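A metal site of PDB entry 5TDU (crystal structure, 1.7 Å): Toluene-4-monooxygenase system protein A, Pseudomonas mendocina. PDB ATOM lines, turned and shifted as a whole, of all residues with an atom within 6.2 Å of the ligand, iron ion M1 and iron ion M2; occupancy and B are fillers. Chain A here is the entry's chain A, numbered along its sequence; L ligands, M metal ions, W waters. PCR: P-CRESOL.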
ATOM      1  N   ALA A  99     -36.793 -17.749  -1.862  1.00  0.00           N
ATOM      2  CA  ALA A  99     -36.667 -19.125  -2.338  1.00  0.00           C
ATOM      3  C   ALA A  99     -35.505 -19.293  -3.299  1.00  0.00           C
ATOM      4  O   ALA A  99     -35.037 -20.405  -3.520  1.00  0.00           O
ATOM      5  CB  ALA A  99     -37.955 -19.562  -2.982  1.00  0.00           C
ATOM      6  N   ILE A 100     -34.990 -18.189  -3.832  1.00  0.00           N
ATOM      7  CA  ILE A 100     -34.046 -18.246  -4.953  1.00  0.00           C
ATOM      8  C   ILE A 100     -32.644 -17.723  -4.642  1.00  0.00           C
ATOM      9  O   ILE A 100     -31.642 -18.315  -5.041  1.00  0.00           O
ATOM     10  CB  ILE A 100     -34.633 -17.480  -6.167  1.00  0.00           C
ATOM     11  CG1 ILE A 100     -35.859 -18.213  -6.726  1.00  0.00           C
ATOM     12  CG2 ILE A 100     -33.572 -17.263  -7.239  1.00  0.00           C
ATOM     13  CD1 ILE A 100     -35.556 -19.582  -7.338  1.00  0.00           C
ATOM     14  N   GLY A 103     -30.060 -19.990  -3.014  1.00  0.00           N
ATOM     15  CA  GLY A 103     -29.983 -21.176  -3.865  1.00  0.00           C
ATOM     16  C   GLY A 103     -29.138 -20.918  -5.112  1.00  0.00           C
ATOM     17  O   GLY A 103     -28.391 -21.799  -5.575  1.00  0.00           O
ATOM     18  N   GLU A 104     -29.266 -19.721  -5.673  1.00  0.00           N
ATOM     19  CA  GLU A 104     -28.373 -19.301  -6.760  1.00  0.00           C
ATOM     20  C   GLU A 104     -26.919 -19.410  -6.314  1.00  0.00           C
ATOM     21  O   GLU A 104     -26.055 -19.890  -7.037  1.00  0.00           O
ATOM     22  CB  GLU A 104     -28.659 -17.866  -7.196  1.00  0.00           C
ATOM     23  CG  GLU A 104     -30.038 -17.648  -7.777  1.00  0.00           C
ATOM     24  CD  GLU A 104     -30.055 -17.716  -9.289  1.00  0.00           C
ATOM     25  OE1 GLU A 104     -30.966 -17.126  -9.899  1.00  0.00           O
ATOM     26  OE2 GLU A 104     -29.155 -18.359  -9.864  1.00  0.00           O
ATOM     27  N   TYR A 105     -26.640 -18.899  -5.125  1.00  0.00           N
ATOM     28  CA  TYR A 105     -25.281 -18.949  -4.619  1.00  0.00           C
ATOM     29  C   TYR A 105     -24.854 -20.408  -4.432  1.00  0.00           C
ATOM     30  O   TYR A 105     -23.684 -20.750  -4.671  1.00  0.00           O
ATOM     31  CB  TYR A 105     -25.126 -18.161  -3.307  1.00  0.00           C
ATOM     32  CG  TYR A 105     -23.674 -18.111  -2.888  1.00  0.00           C
ATOM     33  CD1 TYR A 105     -22.778 -17.301  -3.583  1.00  0.00           C
ATOM     34  CD2 TYR A 105     -23.195 -18.898  -1.846  1.00  0.00           C
ATOM     35  CE1 TYR A 105     -21.443 -17.275  -3.228  1.00  0.00           C
ATOM     36  CE2 TYR A 105     -21.868 -18.861  -1.486  1.00  0.00           C
ATOM     37  CZ  TYR A 105     -20.995 -18.055  -2.189  1.00  0.00           C
ATOM     38  OH  TYR A 105     -19.662 -18.025  -1.843  1.00  0.00           O
ATOM     39  N   ALA A 107     -25.741 -22.725  -6.335  1.00  0.00           N
ATOM     40  CA  ALA A 107     -25.476 -23.253  -7.666  1.00  0.00           C
ATOM     41  C   ALA A 107     -24.027 -23.028  -8.099  1.00  0.00           C
ATOM     42  O   ALA A 107     -23.522 -23.730  -8.973  1.00  0.00           O
ATOM     43  CB  ALA A 107     -26.448 -22.640  -8.688  1.00  0.00           C
ATOM     44  N   GLU A 111     -21.650 -25.820 -10.215  1.00  0.00           N
ATOM     45  CA  GLU A 111     -20.773 -25.449 -11.306  1.00  0.00           C
ATOM     46  C   GLU A 111     -19.318 -25.751 -10.921  1.00  0.00           C
ATOM     47  O   GLU A 111     -18.547 -26.272 -11.730  1.00  0.00           O
ATOM     48  CB  GLU A 111     -20.954 -23.964 -11.655  1.00  0.00           C
ATOM     49  CG  GLU A 111     -22.323 -23.636 -12.284  1.00  0.00           C
ATOM     50  CD  GLU A 111     -22.468 -24.121 -13.734  1.00  0.00           C
ATOM     51  OE1 GLU A 111     -21.457 -24.508 -14.329  1.00  0.00           O
ATOM     52  OE2 GLU A 111     -23.600 -24.086 -14.273  1.00  0.00           O
ATOM     53  N   ASP A 133     -21.400 -16.867 -13.254  1.00  0.00           N
ATOM     54  CA  ASP A 133     -22.795 -16.502 -13.476  1.00  0.00           C
ATOM     55  C   ASP A 133     -23.614 -16.633 -12.208  1.00  0.00           C
ATOM     56  O   ASP A 133     -24.422 -15.770 -11.882  1.00  0.00           O
ATOM     57  CB  ASP A 133     -23.462 -17.388 -14.542  1.00  0.00           C
ATOM     58  CG  ASP A 133     -22.907 -17.171 -15.938  1.00  0.00           C
ATOM     59  OD1 ASP A 133     -22.293 -16.104 -16.221  1.00  0.00           O
ATOM     60  OD2 ASP A 133     -23.117 -18.073 -16.765  1.00  0.00           O
ATOM     61  N   GLU A 134     -23.472 -17.762 -11.505  1.00  0.00           N
ATOM     62  CA  GLU A 134     -24.325 -17.996 -10.356  1.00  0.00           C
ATOM     63  C   GLU A 134     -23.934 -17.060  -9.213  1.00  0.00           C
ATOM     64  O   GLU A 134     -24.769 -16.667  -8.408  1.00  0.00           O
ATOM     65  CB  GLU A 134     -24.253 -19.456  -9.904  1.00  0.00           C
ATOM     66  CG  GLU A 134     -24.659 -20.487 -10.982  1.00  0.00           C
ATOM     67  CD  GLU A 134     -26.092 -20.338 -11.493  1.00  0.00           C
ATOM     68  OE1 GLU A 134     -26.771 -19.321 -11.207  1.00  0.00           O
ATOM     69  OE2 GLU A 134     -26.553 -21.269 -12.180  1.00  0.00           O
ATOM     70  N   HIS A 137     -25.822 -14.056  -9.920  1.00  0.00           N
ATOM     71  CA  HIS A 137     -27.249 -14.227  -9.654  1.00  0.00           C
ATOM     72  C   HIS A 137     -27.535 -14.178  -8.162  1.00  0.00           C
ATOM     73  O   HIS A 137     -28.533 -13.593  -7.744  1.00  0.00           O
ATOM     74  CB  HIS A 137     -27.747 -15.546 -10.251  1.00  0.00           C
ATOM     75  CG  HIS A 137     -27.565 -15.610 -11.742  1.00  0.00           C
ATOM     76  ND1 HIS A 137     -27.800 -16.753 -12.480  1.00  0.00           N
ATOM     77  CD2 HIS A 137     -27.158 -14.667 -12.628  1.00  0.00           C
ATOM     78  CE1 HIS A 137     -27.557 -16.514 -13.761  1.00  0.00           C
ATOM     79  NE2 HIS A 137     -27.158 -15.245 -13.878  1.00  0.00           N
ATOM     80  N   GLN A 141     -29.606 -10.976  -6.390  1.00  0.00           N
ATOM     81  CA  GLN A 141     -30.889 -11.246  -5.775  1.00  0.00           C
ATOM     82  C   GLN A 141     -30.835 -11.134  -4.253  1.00  0.00           C
ATOM     83  O   GLN A 141     -31.843 -11.330  -3.582  1.00  0.00           O
ATOM     84  CB  GLN A 141     -31.396 -12.595  -6.252  1.00  0.00           C
ATOM     85  CG  GLN A 141     -31.932 -12.456  -7.685  1.00  0.00           C
ATOM     86  CD  GLN A 141     -32.261 -13.765  -8.361  1.00  0.00           C
ATOM     87  OE1 GLN A 141     -33.396 -13.994  -8.750  1.00  0.00           O
ATOM     88  NE2 GLN A 141     -31.244 -14.611  -8.523  1.00  0.00           N
ATOM     89  N   TYR A 162     -32.703 -19.765   3.574  1.00  0.00           N
ATOM     90  CA  TYR A 162     -31.913 -21.003   3.479  1.00  0.00           C
ATOM     91  C   TYR A 162     -31.177 -21.318   4.771  1.00  0.00           C
ATOM     92  O   TYR A 162     -30.668 -22.422   4.946  1.00  0.00           O
ATOM     93  CB  TYR A 162     -30.913 -20.929   2.322  1.00  0.00           C
ATOM     94  CG  TYR A 162     -31.515 -21.246   0.968  1.00  0.00           C
ATOM     95  CD1 TYR A 162     -32.530 -20.465   0.415  1.00  0.00           C
ATOM     96  CD2 TYR A 162     -31.047 -22.330   0.229  1.00  0.00           C
ATOM     97  CE1 TYR A 162     -33.066 -20.767  -0.826  1.00  0.00           C
ATOM     98  CE2 TYR A 162     -31.576 -22.629  -1.022  1.00  0.00           C
ATOM     99  CZ  TYR A 162     -32.583 -21.840  -1.542  1.00  0.00           C
ATOM    100  OH  TYR A 162     -33.097 -22.125  -2.780  1.00  0.00           O
ATOM    101  N   PHE A 176     -32.441 -28.601  -4.096  1.00  0.00           N
ATOM    102  CA  PHE A 176     -31.190 -28.074  -4.632  1.00  0.00           C
ATOM    103  C   PHE A 176     -29.988 -28.850  -4.119  1.00  0.00           C
ATOM    104  O   PHE A 176     -29.007 -29.048  -4.845  1.00  0.00           O
ATOM    105  CB  PHE A 176     -31.071 -26.577  -4.315  1.00  0.00           C
ATOM    106  CG  PHE A 176     -32.026 -25.749  -5.099  1.00  0.00           C
ATOM    107  CD1 PHE A 176     -32.118 -25.913  -6.483  1.00  0.00           C
ATOM    108  CD2 PHE A 176     -32.862 -24.842  -4.482  1.00  0.00           C
ATOM    109  CE1 PHE A 176     -33.011 -25.173  -7.224  1.00  0.00           C
ATOM    110  CE2 PHE A 176     -33.753 -24.093  -5.219  1.00  0.00           C
ATOM    111  CZ  PHE A 176     -33.842 -24.264  -6.584  1.00  0.00           C
ATOM    112  N   ILE A 180     -28.010 -30.134  -7.111  1.00  0.00           N
ATOM    113  CA  ILE A 180     -26.916 -29.182  -7.345  1.00  0.00           C
ATOM    114  C   ILE A 180     -25.659 -29.528  -6.552  1.00  0.00           C
ATOM    115  O   ILE A 180     -24.590 -29.675  -7.123  1.00  0.00           O
ATOM    116  CB  ILE A 180     -27.339 -27.746  -7.001  1.00  0.00           C
ATOM    117  CG1 ILE A 180     -28.558 -27.327  -7.837  1.00  0.00           C
ATOM    118  CG2 ILE A 180     -26.163 -26.780  -7.190  1.00  0.00           C
ATOM    119  CD1 ILE A 180     -28.888 -25.843  -7.708  1.00  0.00           C
ATOM    120  N   LEU A 192     -29.020 -30.496 -13.107  1.00  0.00           N
ATOM    121  CA  LEU A 192     -29.059 -29.042 -12.995  1.00  0.00           C
ATOM    122  C   LEU A 192     -29.060 -28.361 -14.363  1.00  0.00           C
ATOM    123  O   LEU A 192     -30.048 -27.715 -14.723  1.00  0.00           O
ATOM    124  CB  LEU A 192     -27.880 -28.533 -12.166  1.00  0.00           C
ATOM    125  CG  LEU A 192     -27.724 -27.007 -12.136  1.00  0.00           C
ATOM    126  CD1 LEU A 192     -28.981 -26.349 -11.560  1.00  0.00           C
ATOM    127  CD2 LEU A 192     -26.479 -26.630 -11.323  1.00  0.00           C
ATOM    128  N   PHE A 196     -33.059 -28.802 -15.033  1.00  0.00           N
ATOM    129  CA  PHE A 196     -33.616 -27.668 -14.304  1.00  0.00           C
ATOM    130  C   PHE A 196     -33.469 -26.359 -15.076  1.00  0.00           C
ATOM    131  O   PHE A 196     -34.418 -25.586 -15.201  1.00  0.00           O
ATOM    132  CB  PHE A 196     -32.967 -27.559 -12.927  1.00  0.00           C
ATOM    133  CG  PHE A 196     -33.520 -26.462 -12.061  1.00  0.00           C
ATOM    134  CD1 PHE A 196     -34.838 -26.496 -11.623  1.00  0.00           C
ATOM    135  CD2 PHE A 196     -32.706 -25.393 -11.664  1.00  0.00           C
ATOM    136  CE1 PHE A 196     -35.349 -25.482 -10.816  1.00  0.00           C
ATOM    137  CE2 PHE A 196     -33.208 -24.392 -10.853  1.00  0.00           C
ATOM    138  CZ  PHE A 196     -34.528 -24.432 -10.427  1.00  0.00           C
ATOM    139  N   GLU A 197     -32.266 -26.122 -15.614  1.00  0.00           N
ATOM    140  CA  GLU A 197     -31.933 -24.807 -16.178  1.00  0.00           C
ATOM    141  C   GLU A 197     -32.346 -24.591 -17.647  1.00  0.00           C
ATOM    142  O   GLU A 197     -32.434 -23.441 -18.092  1.00  0.00           O
ATOM    143  CB  GLU A 197     -30.417 -24.566 -16.034  1.00  0.00           C
ATOM    144  CG  GLU A 197     -29.993 -24.380 -14.590  1.00  0.00           C
ATOM    145  CD  GLU A 197     -28.509 -24.073 -14.438  1.00  0.00           C
ATOM    146  OE1 GLU A 197     -27.691 -24.627 -15.202  1.00  0.00           O
ATOM    147  OE2 GLU A 197     -28.154 -23.264 -13.562  1.00  0.00           O
ATOM    148  N   THR A 201     -36.505 -23.251 -15.074  1.00  0.00           N
ATOM    149  CA  THR A 201     -36.244 -21.892 -14.605  1.00  0.00           C
ATOM    150  C   THR A 201     -36.867 -20.836 -15.523  1.00  0.00           C
ATOM    151  O   THR A 201     -37.156 -19.725 -15.074  1.00  0.00           O
ATOM    152  CB  THR A 201     -34.739 -21.590 -14.447  1.00  0.00           C
ATOM    153  OG1 THR A 201     -34.060 -21.834 -15.679  1.00  0.00           O
ATOM    154  CG2 THR A 201     -34.140 -22.483 -13.368  1.00  0.00           C
ATOM    155  N   PHE A 205     -38.274 -17.157 -14.271  1.00  0.00           N
ATOM    156  CA  PHE A 205     -37.459 -16.013 -14.656  1.00  0.00           C
ATOM    157  C   PHE A 205     -37.910 -15.344 -15.962  1.00  0.00           C
ATOM    158  O   PHE A 205     -37.437 -14.247 -16.296  1.00  0.00           O
ATOM    159  CB  PHE A 205     -35.983 -16.414 -14.774  1.00  0.00           C
ATOM    160  CG  PHE A 205     -35.334 -16.733 -13.459  1.00  0.00           C
ATOM    161  CD1 PHE A 205     -35.516 -17.961 -12.845  1.00  0.00           C
ATOM    162  CD2 PHE A 205     -34.524 -15.786 -12.826  1.00  0.00           C
ATOM    163  CE1 PHE A 205     -34.915 -18.249 -11.629  1.00  0.00           C
ATOM    164  CE2 PHE A 205     -33.923 -16.062 -11.615  1.00  0.00           C
ATOM    165  CZ  PHE A 205     -34.118 -17.295 -11.012  1.00  0.00           C
ATOM    166  N   ILE A 227     -30.842 -12.087 -15.874  1.00  0.00           N
ATOM    167  CA  ILE A 227     -30.292 -13.285 -15.255  1.00  0.00           C
ATOM    168  C   ILE A 227     -30.450 -14.490 -16.191  1.00  0.00           C
ATOM    169  O   ILE A 227     -29.531 -15.301 -16.345  1.00  0.00           O
ATOM    170  CB  ILE A 227     -30.980 -13.534 -13.891  1.00  0.00           C
ATOM    171  CG1 ILE A 227     -30.435 -12.538 -12.871  1.00  0.00           C
ATOM    172  CG2 ILE A 227     -30.767 -14.991 -13.451  1.00  0.00           C
ATOM    173  CD1 ILE A 227     -31.131 -12.551 -11.505  1.00  0.00           C
ATOM    174  N   ASP A 230     -27.861 -15.402 -18.869  1.00  0.00           N
ATOM    175  CA  ASP A 230     -26.707 -16.198 -18.430  1.00  0.00           C
ATOM    176  C   ASP A 230     -27.057 -17.677 -18.378  1.00  0.00           C
ATOM    177  O   ASP A 230     -26.293 -18.526 -18.821  1.00  0.00           O
ATOM    178  CB  ASP A 230     -26.251 -15.788 -17.029  1.00  0.00           C
ATOM    179  CG  ASP A 230     -25.775 -14.354 -16.947  1.00  0.00           C
ATOM    180  OD1 ASP A 230     -25.191 -13.832 -17.933  1.00  0.00           O
ATOM    181  OD2 ASP A 230     -25.992 -13.748 -15.866  1.00  0.00           O
ATOM    182  N   GLU A 231     -28.209 -17.957 -17.767  1.00  0.00           N
ATOM    183  CA  GLU A 231     -28.758 -19.304 -17.697  1.00  0.00           C
ATOM    184  C   GLU A 231     -28.717 -19.954 -19.066  1.00  0.00           C
ATOM    185  O   GLU A 231     -28.295 -21.119 -19.234  1.00  0.00           O
ATOM    186  CB  GLU A 231     -30.194 -19.252 -17.174  1.00  0.00           C
ATOM    187  CG  GLU A 231     -30.840 -20.619 -16.965  1.00  0.00           C
ATOM    188  CD  GLU A 231     -30.577 -21.167 -15.582  1.00  0.00           C
ATOM    189  OE1 GLU A 231     -31.555 -21.524 -14.889  1.00  0.00           O
ATOM    190  OE2 GLU A 231     -29.394 -21.228 -15.179  1.00  0.00           O
ATOM    191  N   HIS A 234     -24.992 -21.051 -19.803  1.00  0.00           N
ATOM    192  CA  HIS A 234     -24.336 -22.136 -19.063  1.00  0.00           C
ATOM    193  C   HIS A 234     -25.209 -23.399 -18.960  1.00  0.00           C
ATOM    194  O   HIS A 234     -24.695 -24.498 -18.709  1.00  0.00           O
ATOM    195  CB  HIS A 234     -23.833 -21.671 -17.660  1.00  0.00           C
ATOM    196  CG  HIS A 234     -24.898 -21.280 -16.676  1.00  0.00           C
ATOM    197  ND1 HIS A 234     -24.920 -20.036 -16.083  1.00  0.00           N
ATOM    198  CD2 HIS A 234     -25.902 -21.986 -16.107  1.00  0.00           C
ATOM    199  CE1 HIS A 234     -25.918 -19.977 -15.222  1.00  0.00           C
ATOM    200  NE2 HIS A 234     -26.536 -21.152 -15.216  1.00  0.00           N
ATOM    201  N   ALA A 235     -26.508 -23.278 -19.202  1.00  0.00           N
ATOM    202  CA  ALA A 235     -27.387 -24.470 -19.212  1.00  0.00           C
ATOM    203  C   ALA A 235     -27.021 -25.406 -20.365  1.00  0.00           C
ATOM    204  O   ALA A 235     -27.338 -26.610 -20.324  1.00  0.00           O
ATOM    205  CB  ALA A 235     -28.872 -24.054 -19.292  1.00  0.00           C
HETATM  206  CB  PCR L   1     -32.411 -21.855  -7.330  1.00  0.00           C
HETATM  207  CG  PCR L   1     -31.629 -21.594  -8.587  1.00  0.00           C
HETATM  208  CD1 PCR L   1     -30.411 -22.161  -8.690  1.00  0.00           C
HETATM  209  CE1 PCR L   1     -29.679 -21.942  -9.770  1.00  0.00           C
HETATM  210  CD2 PCR L   1     -32.128 -20.794  -9.534  1.00  0.00           C
HETATM  211  CE2 PCR L   1     -31.391 -20.540 -10.656  1.00  0.00           C
HETATM  212  CZ  PCR L   1     -30.150 -21.115 -10.745  1.00  0.00           C
HETATM  213  OH  PCR L   1     -29.391 -20.890 -11.795  1.00  0.00           O
HETATM  214 FE    FE M   1     -28.141 -21.285 -13.632  1.00  0.00          FE
HETATM  215 FE    FE M   2     -28.679 -18.659 -11.869  1.00  0.00          FE
HETATM  216  O   HOH W   1     -30.743 -18.007 -12.335  1.00  0.00           O
HETATM  217  O   HOH W   2     -28.509 -19.236 -14.043  1.00  0.00           O
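Merely in contact with the ligand: Phe 176 (2.9 Å), Ala 107 (3.5 Å), Gly 103 (3.7 Å), Ile 100 (3.9 Å) and Phe 196 (3.9 Å).
Hydrophobic or aromatic side chains within 4 Å of the ligand: Ile 100, Ala 107, Phe 176 and Phe 196.
Within 4 Å of the ligand: Ile 100, Gly 103, Glu 104, Ala 107, Glu 134, Phe 176, Phe 196, Glu 197 and Glu 231.
The nearest printed residue that does not touch the ligand is Ile 180 (4.1 Å).
Iron ion M1 is bound by OE2 of Glu 197 (2.0 Å), OE2 of Glu 231 (2.0 Å), water W2 (2.1 Å), OE2 of Glu 134 (2.2 Å), OH of the ligand (2.3 Å) and NE2 of His 234 (2.3 Å).
Iron ion M2 is bound by the side-chain carboxylate of Glu 104 (2.1 Å), the side-chain carboxylate of Glu 134 (2.1 Å), a ring nitrogen (ND1) of His 137 (2.2 Å), water W1 (2.2 Å), water W2 (2.3 Å) and an oxygen (OH) of the ligand (2.3 Å).
Iron ion M2 has six donor atoms within binding distance.
Along chain A the residues within 4 Å of iron ion M2 span positions 104 to 137.
Four residues have an atom within 4 Å of iron ion M1: Glu 134, Glu 197, Glu 231 and His 234.
The backbone NH of Glu 197 sits at hydrogen-bond distance from the backbone carbonyl oxygen of Leu 192 (2.9 Å).
OE1 of Glu 231 sits at hydrogen-bond distance from OG1 of Thr 201, at 2.6 Å.
A ring nitrogen (NE2) of His 137 is in hydrogen-bond range of the backbone carbonyl oxygen of Ile 227, 3.4 Å away.
NE2 of His 137 sits close to O of Asp 133, 3.4 Å away.
The backbone carbonyl oxygen (O) of His 137 is in hydrogen-bond range of the side-chain amide nitrogen (NE2) of Gln 141, at 3.0 Å.
OD2 of Asp 230 lies within hydrogen-bond range of NE2 of His 137 (2.7 Å).
A ring nitrogen (ND1) of His 234 lies within hydrogen-bond range of the side-chain carboxylate (OD2) of Asp 133 (2.8 Å).
ND1 of His 234 sits at hydrogen-bond distance from O of Asp 230, 3.4 Å away.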
